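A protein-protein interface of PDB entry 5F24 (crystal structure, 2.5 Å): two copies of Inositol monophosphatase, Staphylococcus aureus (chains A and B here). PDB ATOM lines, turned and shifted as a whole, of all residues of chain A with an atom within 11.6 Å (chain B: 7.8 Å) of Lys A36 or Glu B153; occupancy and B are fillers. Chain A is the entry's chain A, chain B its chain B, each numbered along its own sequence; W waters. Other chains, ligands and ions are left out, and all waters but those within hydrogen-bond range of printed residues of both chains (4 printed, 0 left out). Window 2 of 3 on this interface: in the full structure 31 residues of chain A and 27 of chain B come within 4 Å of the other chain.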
ATOM      1  N   MET A  31      19.193  27.201 -26.810  1.00  0.00           N
ATOM      2  CA  MET A  31      18.829  26.018 -25.981  1.00  0.00           C
ATOM      3  C   MET A  31      17.290  25.880 -25.944  1.00  0.00           C
ATOM      4  O   MET A  31      16.676  25.280 -26.844  1.00  0.00           O
ATOM      5  CB  MET A  31      19.451  26.096 -24.538  1.00  0.00           C
ATOM      6  CG  MET A  31      18.486  25.801 -23.378  1.00  0.00           C
ATOM      7  SD  MET A  31      19.105  25.902 -21.659  1.00  0.00           S
ATOM      8  CE  MET A  31      17.703  25.266 -20.788  1.00  0.00           C
ATOM      9  N   THR A  33      17.168  22.628 -26.965  1.00  0.00           N
ATOM     10  CA  THR A  33      15.942  21.829 -27.080  1.00  0.00           C
ATOM     11  C   THR A  33      16.112  20.282 -26.842  1.00  0.00           C
ATOM     12  O   THR A  33      15.111  19.588 -26.641  1.00  0.00           O
ATOM     13  CB  THR A  33      15.247  22.120 -28.448  1.00  0.00           C
ATOM     14  N   GLU A  34      17.359  19.758 -26.850  1.00  0.00           N
ATOM     15  CA  GLU A  34      17.685  18.280 -26.773  1.00  0.00           C
ATOM     16  C   GLU A  34      17.656  17.610 -25.342  1.00  0.00           C
ATOM     17  O   GLU A  34      17.889  18.297 -24.351  1.00  0.00           O
ATOM     18  CB  GLU A  34      19.075  18.001 -27.431  1.00  0.00           C
ATOM     19  N   THR A  35      17.369  16.301 -25.190  1.00  0.00           N
ATOM     20  CA  THR A  35      16.717  15.373 -26.169  1.00  0.00           C
ATOM     21  C   THR A  35      17.548  14.208 -26.735  1.00  0.00           C
ATOM     22  O   THR A  35      17.054  13.541 -27.674  1.00  0.00           O
ATOM     23  CB  THR A  35      15.892  16.030 -27.330  1.00  0.00           C
ATOM     24  N   LYS A  36      18.802  14.076 -26.248  1.00  0.00           N
ATOM     25  CA  LYS A  36      19.468  12.761 -26.024  1.00  0.00           C
ATOM     26  C   LYS A  36      20.965  12.828 -25.623  1.00  0.00           C
ATOM     27  O   LYS A  36      21.862  12.421 -26.387  1.00  0.00           O
ATOM     28  CB  LYS A  36      19.211  11.711 -27.127  1.00  0.00           C
ATOM     29  CG  LYS A  36      18.124  10.704 -26.735  1.00  0.00           C
ATOM     30  CD  LYS A  36      17.891   9.644 -27.807  1.00  0.00           C
ATOM     31  CE  LYS A  36      19.050   8.660 -27.963  1.00  0.00           C
ATOM     32  NZ  LYS A  36      20.383   9.291 -27.825  1.00  0.00           N
ATOM     33  N   ARG A  37      21.182  13.346 -24.402  1.00  0.00           N
ATOM     34  CA  ARG A  37      22.356  13.109 -23.555  1.00  0.00           C
ATOM     35  C   ARG A  37      21.819  12.719 -22.155  1.00  0.00           C
ATOM     36  O   ARG A  37      20.795  13.245 -21.710  1.00  0.00           O
ATOM     37  CB  ARG A  37      23.225  14.342 -23.426  1.00  0.00           C
ATOM     38  CG  ARG A  37      24.017  14.660 -24.674  1.00  0.00           C
ATOM     39  CD  ARG A  37      24.817  15.936 -24.506  1.00  0.00           C
ATOM     40  NE  ARG A  37      25.010  16.598 -25.795  1.00  0.00           N
ATOM     41  CZ  ARG A  37      25.908  17.553 -26.043  1.00  0.00           C
ATOM     42  NH1 ARG A  37      26.732  17.987 -25.084  1.00  0.00           N
ATOM     43  NH2 ARG A  37      25.989  18.077 -27.267  1.00  0.00           N
ATOM     44  N   HIS A  38      22.481  11.793 -21.466  1.00  0.00           N
ATOM     45  CA  HIS A  38      22.026  11.423 -20.131  1.00  0.00           C
ATOM     46  C   HIS A  38      22.498  12.411 -19.029  1.00  0.00           C
ATOM     47  O   HIS A  38      23.280  13.353 -19.276  1.00  0.00           O
ATOM     48  CB  HIS A  38      22.395   9.974 -19.784  1.00  0.00           C
ATOM     49  CG  HIS A  38      23.868   9.720 -19.684  1.00  0.00           C
ATOM     50  ND1 HIS A  38      24.517   8.808 -20.479  1.00  0.00           N
ATOM     51  CD2 HIS A  38      24.815  10.247 -18.873  1.00  0.00           C
ATOM     52  CE1 HIS A  38      25.796   8.787 -20.158  1.00  0.00           C
ATOM     53  NE2 HIS A  38      26.002   9.654 -19.193  1.00  0.00           N
ATOM     54  N   ARG A  39      21.993  12.150 -17.820  1.00  0.00           N
ATOM     55  CA  ARG A  39      22.158  13.003 -16.622  1.00  0.00           C
ATOM     56  C   ARG A  39      23.593  13.546 -16.458  1.00  0.00           C
ATOM     57  O   ARG A  39      23.785  14.717 -16.135  1.00  0.00           O
ATOM     58  CB  ARG A  39      21.723  12.194 -15.373  1.00  0.00           C
ATOM     59  CG  ARG A  39      21.457  12.994 -14.120  1.00  0.00           C
ATOM     60  CD  ARG A  39      21.891  12.253 -12.841  1.00  0.00           C
ATOM     61  NE  ARG A  39      21.374  10.885 -12.746  1.00  0.00           N
ATOM     62  CZ  ARG A  39      20.120  10.531 -12.418  1.00  0.00           C
ATOM     63  NH1 ARG A  39      19.775   9.257 -12.360  1.00  0.00           N
ATOM     64  NH2 ARG A  39      19.196  11.425 -12.149  1.00  0.00           N
ATOM     65  N   PHE A  40      24.575  12.680 -16.695  1.00  0.00           N
ATOM     66  CA  PHE A  40      26.002  12.968 -16.422  1.00  0.00           C
ATOM     67  C   PHE A  40      26.724  13.770 -17.493  1.00  0.00           C
ATOM     68  O   PHE A  40      27.816  14.262 -17.254  1.00  0.00           O
ATOM     69  CB  PHE A  40      26.745  11.647 -16.156  1.00  0.00           C
ATOM     70  CG  PHE A  40      26.182  10.903 -14.985  1.00  0.00           C
ATOM     71  CD1 PHE A  40      26.399  11.374 -13.691  1.00  0.00           C
ATOM     72  CD2 PHE A  40      25.361   9.802 -15.166  1.00  0.00           C
ATOM     73  CE1 PHE A  40      25.825  10.737 -12.603  1.00  0.00           C
ATOM     74  CE2 PHE A  40      24.797   9.165 -14.084  1.00  0.00           C
ATOM     75  CZ  PHE A  40      25.021   9.637 -12.804  1.00  0.00           C
ATOM     76  N   ASP A  41      26.085  13.923 -18.652  1.00  0.00           N
ATOM     77  CA  ASP A  41      26.720  14.472 -19.831  1.00  0.00           C
ATOM     78  C   ASP A  41      26.135  15.805 -20.339  1.00  0.00           C
ATOM     79  O   ASP A  41      26.277  16.120 -21.527  1.00  0.00           O
ATOM     80  CB  ASP A  41      26.683  13.398 -20.937  1.00  0.00           C
ATOM     81  CG  ASP A  41      27.799  12.369 -20.794  1.00  0.00           C
ATOM     82  OD1 ASP A  41      28.579  12.477 -19.819  1.00  0.00           O
ATOM     83  OD2 ASP A  41      27.895  11.477 -21.668  1.00  0.00           O
ATOM     84  N   LEU A  42      25.537  16.596 -19.443  1.00  0.00           N
ATOM     85  CA  LEU A  42      24.835  17.849 -19.822  1.00  0.00           C
ATOM     86  C   LEU A  42      25.754  19.087 -19.989  1.00  0.00           C
ATOM     87  O   LEU A  42      26.787  19.217 -19.314  1.00  0.00           O
ATOM     88  CB  LEU A  42      23.739  18.171 -18.787  1.00  0.00           C
ATOM     89  CG  LEU A  42      22.454  17.340 -18.774  1.00  0.00           C
ATOM     90  CD1 LEU A  42      21.650  17.779 -17.563  1.00  0.00           C
ATOM     91  CD2 LEU A  42      21.630  17.480 -20.044  1.00  0.00           C
ATOM     92  N   VAL A  43      25.336  20.021 -20.846  1.00  0.00           N
ATOM     93  CA  VAL A  43      26.180  21.190 -21.218  1.00  0.00           C
ATOM     94  C   VAL A  43      26.372  22.265 -20.056  1.00  0.00           C
ATOM     95  O   VAL A  43      27.275  22.077 -19.199  1.00  0.00           O
ATOM     96  CB  VAL A  43      25.839  21.678 -22.665  1.00  0.00           C
ATOM     97  CG1 VAL A  43      26.626  20.875 -23.711  1.00  0.00           C
ATOM     98  CG2 VAL A  43      24.345  21.576 -22.934  1.00  0.00           C
ATOM     99  N   ALA A  94      20.229  19.673 -14.751  1.00  0.00           N
ATOM    100  CA  ALA A  94      19.252  18.743 -15.296  1.00  0.00           C
ATOM    101  C   ALA A  94      17.877  19.388 -15.270  1.00  0.00           C
ATOM    102  O   ALA A  94      17.176  19.367 -16.282  1.00  0.00           O
ATOM    103  CB  ALA A  94      19.244  17.446 -14.515  1.00  0.00           C
ATOM    104  N   VAL A  97      17.577  22.159 -17.930  1.00  0.00           N
ATOM    105  CA  VAL A  97      17.417  21.639 -19.285  1.00  0.00           C
ATOM    106  C   VAL A  97      16.045  20.989 -19.503  1.00  0.00           C
ATOM    107  O   VAL A  97      15.382  21.267 -20.478  1.00  0.00           O
ATOM    108  CB  VAL A  97      18.543  20.602 -19.622  1.00  0.00           C
ATOM    109  CG1 VAL A  97      18.312  19.953 -20.987  1.00  0.00           C
ATOM    110  CG2 VAL A  97      19.899  21.275 -19.599  1.00  0.00           C
ATOM    111  N   LYS A  98      15.648  20.174 -18.563  1.00  0.00           N
ATOM    112  CA  LYS A  98      14.371  19.420 -18.666  1.00  0.00           C
ATOM    113  C   LYS A  98      13.167  20.217 -18.305  1.00  0.00           C
ATOM    114  O   LYS A  98      12.098  19.899 -18.784  1.00  0.00           O
ATOM    115  CB  LYS A  98      14.445  18.134 -17.899  1.00  0.00           C
ATOM    116  CG  LYS A  98      15.537  17.240 -18.437  1.00  0.00           C
ATOM    117  CD  LYS A  98      15.323  16.752 -19.866  1.00  0.00           C
ATOM    118  CE  LYS A  98      16.479  15.825 -20.273  1.00  0.00           C
ATOM    119  NZ  LYS A  98      16.370  15.217 -21.633  1.00  0.00           N
ATOM    120  N   GLN A 162      18.491   6.888  -6.022  1.00  0.00           N
ATOM    121  CA  GLN A 162      19.013   6.044  -7.077  1.00  0.00           C
ATOM    122  C   GLN A 162      20.413   5.626  -6.778  1.00  0.00           C
ATOM    123  O   GLN A 162      20.934   4.726  -7.410  1.00  0.00           O
ATOM    124  CB  GLN A 162      19.004   6.784  -8.413  1.00  0.00           C
ATOM    125  CG  GLN A 162      17.648   7.351  -8.776  1.00  0.00           C
ATOM    126  CD  GLN A 162      17.580   7.901 -10.186  1.00  0.00           C
ATOM    127  OE1 GLN A 162      17.269   9.071 -10.383  1.00  0.00           O
ATOM    128  NE2 GLN A 162      17.855   7.067 -11.174  1.00  0.00           N
ATOM    129  N   LEU B 150       8.728  13.131 -25.643  1.00  0.00           N
ATOM    130  CA  LEU B 150       9.749  12.657 -24.724  1.00  0.00           C
ATOM    131  C   LEU B 150       9.747  11.145 -24.638  1.00  0.00           C
ATOM    132  O   LEU B 150       8.806  10.550 -24.123  1.00  0.00           O
ATOM    133  CB  LEU B 150       9.538  13.242 -23.338  1.00  0.00           C
ATOM    134  CG  LEU B 150       9.717  14.762 -23.216  1.00  0.00           C
ATOM    135  CD1 LEU B 150       9.295  15.232 -21.830  1.00  0.00           C
ATOM    136  CD2 LEU B 150      11.135  15.173 -23.557  1.00  0.00           C
ATOM    137  N   LYS B 151      10.804  10.514 -25.130  1.00  0.00           N
ATOM    138  CA  LYS B 151      11.063   9.108 -24.808  1.00  0.00           C
ATOM    139  C   LYS B 151      11.402   8.984 -23.348  1.00  0.00           C
ATOM    140  O   LYS B 151      11.998   9.904 -22.766  1.00  0.00           O
ATOM    141  CB  LYS B 151      12.199   8.545 -25.627  1.00  0.00           C
ATOM    142  CG  LYS B 151      11.904   8.411 -27.095  1.00  0.00           C
ATOM    143  CD  LYS B 151      13.005   7.592 -27.759  1.00  0.00           C
ATOM    144  CE  LYS B 151      13.085   7.889 -29.238  1.00  0.00           C
ATOM    145  NZ  LYS B 151      13.377   6.645 -30.012  1.00  0.00           N
ATOM    146  N   LEU B 152      11.095   7.844 -22.744  1.00  0.00           N
ATOM    147  CA  LEU B 152      11.306   7.680 -21.258  1.00  0.00           C
ATOM    148  C   LEU B 152      12.772   7.961 -20.816  1.00  0.00           C
ATOM    149  O   LEU B 152      13.028   8.662 -19.820  1.00  0.00           O
ATOM    150  CB  LEU B 152      10.851   6.314 -20.759  1.00  0.00           C
ATOM    151  CG  LEU B 152      10.979   6.182 -19.234  1.00  0.00           C
ATOM    152  CD1 LEU B 152      10.187   7.236 -18.468  1.00  0.00           C
ATOM    153  CD2 LEU B 152      10.509   4.813 -18.776  1.00  0.00           C
ATOM    154  N   GLU B 153      13.728   7.504 -21.613  1.00  0.00           N
ATOM    155  CA  GLU B 153      15.162   7.687 -21.295  1.00  0.00           C
ATOM    156  C   GLU B 153      15.609   9.152 -21.250  1.00  0.00           C
ATOM    157  O   GLU B 153      16.667   9.528 -20.706  1.00  0.00           O
ATOM    158  CB  GLU B 153      16.055   6.932 -22.287  1.00  0.00           C
ATOM    159  CG  GLU B 153      16.114   7.524 -23.680  1.00  0.00           C
ATOM    160  CD  GLU B 153      16.935   6.659 -24.649  1.00  0.00           C
ATOM    161  OE1 GLU B 153      16.896   6.927 -25.834  1.00  0.00           O
ATOM    162  OE2 GLU B 153      17.616   5.715 -24.267  1.00  0.00           O
ATOM    163  N   ASP B 154      14.815   9.992 -21.884  1.00  0.00           N
ATOM    164  CA  ASP B 154      15.071  11.464 -21.873  1.00  0.00           C
ATOM    165  C   ASP B 154      14.091  12.215 -20.969  1.00  0.00           C
ATOM    166  O   ASP B 154      14.018  13.444 -21.016  1.00  0.00           O
ATOM    167  CB  ASP B 154      14.925  12.033 -23.276  1.00  0.00           C
ATOM    168  CG  ASP B 154      15.822  11.374 -24.257  1.00  0.00           C
ATOM    169  OD1 ASP B 154      17.028  11.230 -23.961  1.00  0.00           O
ATOM    170  OD2 ASP B 154      15.322  11.010 -25.335  1.00  0.00           O
ATOM    171  N   ALA B 155      13.296  11.493 -20.201  1.00  0.00           N
ATOM    172  CA  ALA B 155      12.282  12.146 -19.387  1.00  0.00           C
ATOM    173  C   ALA B 155      12.479  12.013 -17.864  1.00  0.00           C
ATOM    174  O   ALA B 155      12.963  10.982 -17.338  1.00  0.00           O
ATOM    175  CB  ALA B 155      10.934  11.583 -19.748  1.00  0.00           C
ATOM    176  N   ILE B 156      12.086  13.049 -17.158  1.00  0.00           N
ATOM    177  CA  ILE B 156      12.016  12.952 -15.700  1.00  0.00           C
ATOM    178  C   ILE B 156      10.701  12.266 -15.388  1.00  0.00           C
ATOM    179  O   ILE B 156       9.741  12.582 -16.048  1.00  0.00           O
ATOM    180  CB  ILE B 156      12.090  14.333 -15.067  1.00  0.00           C
ATOM    181  CG1 ILE B 156      13.524  14.809 -15.171  1.00  0.00           C
ATOM    182  CG2 ILE B 156      11.631  14.264 -13.615  1.00  0.00           C
ATOM    183  CD1 ILE B 156      13.681  16.278 -14.894  1.00  0.00           C
ATOM    184  N   ILE B 157      10.652  11.330 -14.436  1.00  0.00           N
ATOM    185  CA  ILE B 157       9.347  10.808 -14.036  1.00  0.00           C
ATOM    186  C   ILE B 157       9.109  10.998 -12.574  1.00  0.00           C
ATOM    187  O   ILE B 157      10.024  11.171 -11.785  1.00  0.00           O
ATOM    188  CB  ILE B 157       9.080   9.351 -14.437  1.00  0.00           C
ATOM    189  CG1 ILE B 157      10.259   8.407 -14.233  1.00  0.00           C
ATOM    190  CG2 ILE B 157       8.922   9.303 -15.951  1.00  0.00           C
ATOM    191  CD1 ILE B 157      10.842   8.386 -12.872  1.00  0.00           C
ATOM    192  N   PHE B 173      13.733   3.849 -12.349  1.00  0.00           N
ATOM    193  CA  PHE B 173      14.999   4.604 -12.207  1.00  0.00           C
ATOM    194  C   PHE B 173      15.924   4.335 -13.389  1.00  0.00           C
ATOM    195  O   PHE B 173      16.396   5.271 -14.037  1.00  0.00           O
ATOM    196  CB  PHE B 173      15.725   4.267 -10.895  1.00  0.00           C
ATOM    197  CG  PHE B 173      15.054   4.782  -9.652  1.00  0.00           C
ATOM    198  CD1 PHE B 173      14.083   5.759  -9.690  1.00  0.00           C
ATOM    199  CD2 PHE B 173      15.474   4.318  -8.435  1.00  0.00           C
ATOM    200  CE1 PHE B 173      13.510   6.217  -8.531  1.00  0.00           C
ATOM    201  CE2 PHE B 173      14.941   4.790  -7.266  1.00  0.00           C
ATOM    202  CZ  PHE B 173      13.965   5.747  -7.307  1.00  0.00           C
ATOM    203  N   ASP B 174      16.180   3.084 -13.703  1.00  0.00           N
ATOM    204  CA  ASP B 174      17.158   2.749 -14.783  1.00  0.00           C
ATOM    205  C   ASP B 174      16.702   3.194 -16.175  1.00  0.00           C
ATOM    206  O   ASP B 174      17.513   3.538 -17.022  1.00  0.00           O
ATOM    207  CB  ASP B 174      17.380   1.236 -14.803  1.00  0.00           C
ATOM    208  CG  ASP B 174      18.025   0.718 -13.529  1.00  0.00           C
ATOM    209  OD1 ASP B 174      18.424   1.514 -12.643  1.00  0.00           O
ATOM    210  OD2 ASP B 174      18.162  -0.518 -13.410  1.00  0.00           O
ATOM    211  N   ALA B 175      15.422   3.126 -16.451  1.00  0.00           N
ATOM    212  CA  ALA B 175      14.894   3.459 -17.789  1.00  0.00           C
ATOM    213  C   ALA B 175      14.655   4.956 -18.031  1.00  0.00           C
ATOM    214  O   ALA B 175      14.441   5.353 -19.175  1.00  0.00           O
ATOM    215  CB  ALA B 175      13.584   2.698 -17.987  1.00  0.00           C
ATOM    216  N   SER B 176      14.651   5.765 -16.976  1.00  0.00           N
ATOM    217  CA  SER B 176      14.208   7.178 -17.141  1.00  0.00           C
ATOM    218  C   SER B 176      15.432   8.051 -17.019  1.00  0.00           C
ATOM    219  O   SER B 176      16.484   7.631 -16.600  1.00  0.00           O
ATOM    220  CB  SER B 176      13.148   7.528 -16.112  1.00  0.00           C
ATOM    221  OG  SER B 176      13.725   7.357 -14.841  1.00  0.00           O
ATOM    222  N   PHE B 177      15.268   9.310 -17.362  1.00  0.00           N
ATOM    223  CA  PHE B 177      16.402  10.269 -17.301  1.00  0.00           C
ATOM    224  C   PHE B 177      16.732  10.551 -15.847  1.00  0.00           C
ATOM    225  O   PHE B 177      17.876  10.536 -15.440  1.00  0.00           O
ATOM    226  CB  PHE B 177      16.030  11.562 -18.050  1.00  0.00           C
ATOM    227  CG  PHE B 177      17.110  12.594 -18.036  1.00  0.00           C
ATOM    228  CD1 PHE B 177      18.120  12.574 -19.000  1.00  0.00           C
ATOM    229  CD2 PHE B 177      17.171  13.546 -17.019  1.00  0.00           C
ATOM    230  CE1 PHE B 177      19.152  13.490 -18.959  1.00  0.00           C
ATOM    231  CE2 PHE B 177      18.198  14.480 -16.981  1.00  0.00           C
ATOM    232  CZ  PHE B 177      19.202  14.443 -17.937  1.00  0.00           C
ATOM    233  N   SER B 178      15.710  10.871 -15.063  1.00  0.00           N
ATOM    234  CA  SER B 178      15.818  11.040 -13.633  1.00  0.00           C
ATOM    235  C   SER B 178      14.435  10.966 -12.956  1.00  0.00           C
ATOM    236  O   SER B 178      13.380  10.777 -13.610  1.00  0.00           O
ATOM    237  CB  SER B 178      16.543  12.331 -13.267  1.00  0.00           C
ATOM    238  OG  SER B 178      17.087  12.187 -11.982  1.00  0.00           O
ATOM    239  N   ALA B 246       5.044   9.920 -26.134  1.00  0.00           N
ATOM    240  CA  ALA B 246       6.175   9.130 -26.519  1.00  0.00           C
ATOM    241  C   ALA B 246       6.746   8.159 -25.460  1.00  0.00           C
ATOM    242  O   ALA B 246       7.598   7.347 -25.788  1.00  0.00           O
ATOM    243  CB  ALA B 246       7.290  10.041 -27.021  1.00  0.00           C
ATOM    244  N   CYS B 247       6.393   8.256 -24.190  1.00  0.00           N
ATOM    245  CA  CYS B 247       6.900   7.397 -23.149  1.00  0.00           C
ATOM    246  C   CYS B 247       5.849   6.577 -22.367  1.00  0.00           C
ATOM    247  O   CYS B 247       6.137   5.786 -21.517  1.00  0.00           O
ATOM    248  CB  CYS B 247       7.734   8.209 -22.154  1.00  0.00           C
ATOM    249  SG  CYS B 247       6.882   9.515 -21.216  1.00  0.00           S
ATOM    250  N   THR B 250       6.119   2.530 -22.674  1.00  0.00           N
ATOM    251  CA  THR B 250       7.278   1.984 -21.993  1.00  0.00           C
ATOM    252  C   THR B 250       7.026   2.004 -20.497  1.00  0.00           C
ATOM    253  O   THR B 250       7.339   1.019 -19.834  1.00  0.00           O
ATOM    254  CB  THR B 250       8.571   2.736 -22.368  1.00  0.00           C
ATOM    255  OG1 THR B 250       8.825   2.601 -23.775  1.00  0.00           O
ATOM    256  CG2 THR B 250       9.760   2.172 -21.581  1.00  0.00           C
HETATM  257  O   HOH W   1      19.841  10.211 -17.253  1.00  0.00           O
HETATM  258  O   HOH W   2      15.980   8.074 -13.633  1.00  0.00           O
HETATM  259  O   HOH W   3      19.321  14.576 -11.938  1.00  0.00           O
HETATM  260  O   HOH W   4      17.975  13.188 -22.654  1.00  0.00           O
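Of the 17 printed residues of chain B, 6 touch a printed residue of chain A.
Hydrophobic or aromatic side chains of chain B within 4 Å of the printed part of chain A: Ile B156, Phe B173 and Phe B177.
Water W4 lies within hydrogen-bond range of OD1 of Asp B154 (2.5 Å), NZ of Lys A98 (2.8 Å) and O of Arg A37 (3.0 Å).
Water W2 lies within hydrogen-bond range of OG of Ser B176 (2.7 Å), O of Phe B173 (2.9 Å), N of Ser B178 (3.2 Å) and NE2 of Gln A162 (3.3 Å).
Water W1 lies within hydrogen-bond range of the backbone carbonyl oxygen (O) of Phe B177 (2.7 Å) and the backbone NH (N) of Arg A39 (3.0 Å).
Water W3 bridges NH2 of Arg A39 (3.2 Å) and OG of Ser B178 (3.3 Å).
No position is printed for both chains.
NE2 of Gln A162 sits close to NH1 of Arg A39.
The backbone carbonyl oxygen (O) of Leu B152 is in hydrogen-bond range of the backbone NH (N) of Phe B177, at 3.4 Å.
O of Ala B175 sits close to N of Glu B153 (3.3 Å).
O of Ala B155 sits at hydrogen-bond distance from N of Phe B177 (2.8 Å).
The backbone carbonyl oxygen of Ser B178 is in hydrogen-bond range of the backbone NH of Ile B157.
The backbone carbonyl oxygen (O) of Phe B173 is in hydrogen-bond range of the side-chain hydroxyl (OG) of Ser B176 (3.5 Å).
Lys A36 touches Glu B153.
Lys A36 touches Asp B154 (CG to OD1, 3.0 Å).
O of Arg A37 touches CE1 of Phe B177, 3.2 Å away.
C of His A38 touches CE1 of Phe B177, at 3.5 Å.
Arg A39 touches Phe B177.
Ala A94 touches Phe B177 (CB to CE2, 3.997 Å).
CB of Lys A98 touches CD1 of Ile B156 (3.6 Å).
Phe B177 touches Lys A98 (CE1 to CE, 3.8 Å).
Gln A162 touches Phe B173 (NE2 to CB, 3.5 Å).
Ser B178 touches Gln A162 (OG to OE1, 3.5 Å).
NZ of Lys A98 sits at hydrogen-bond distance from O of Asp B154, at 3.0 Å.
OG of Ser B178 lies close to NH2 of Arg A39, at 2.2 Å.
Glu A34 touches none of the printed residues of chain B.
Thr A35 touches just one residue of chain B: Asp B154.
Of the printed residues of chain B, Lys A36 touches Glu B153 and Asp B154.
Phe A40 touches none of the printed residues of chain B.
Of the printed residues of chain B, Ala A94 touches Phe B177.
Of the printed residues of chain B, Gln A162 touches Phe B173 (3.5 Å) and Ser B178 (3.5 Å).
No residue of chain A comes within 4 Å of Leu B152.
Of the printed residues of chain A, Glu B153 touches Lys A36.
No residue of chain A comes within 4 Å of Ala B155.
No residue of chain A comes within 4 Å of Ala B175.
Ser B176 touches none of the printed residues of chain A.
The nearest printed residue of chain A that does not touch Phe B177 is Leu A42 (4.2 Å).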
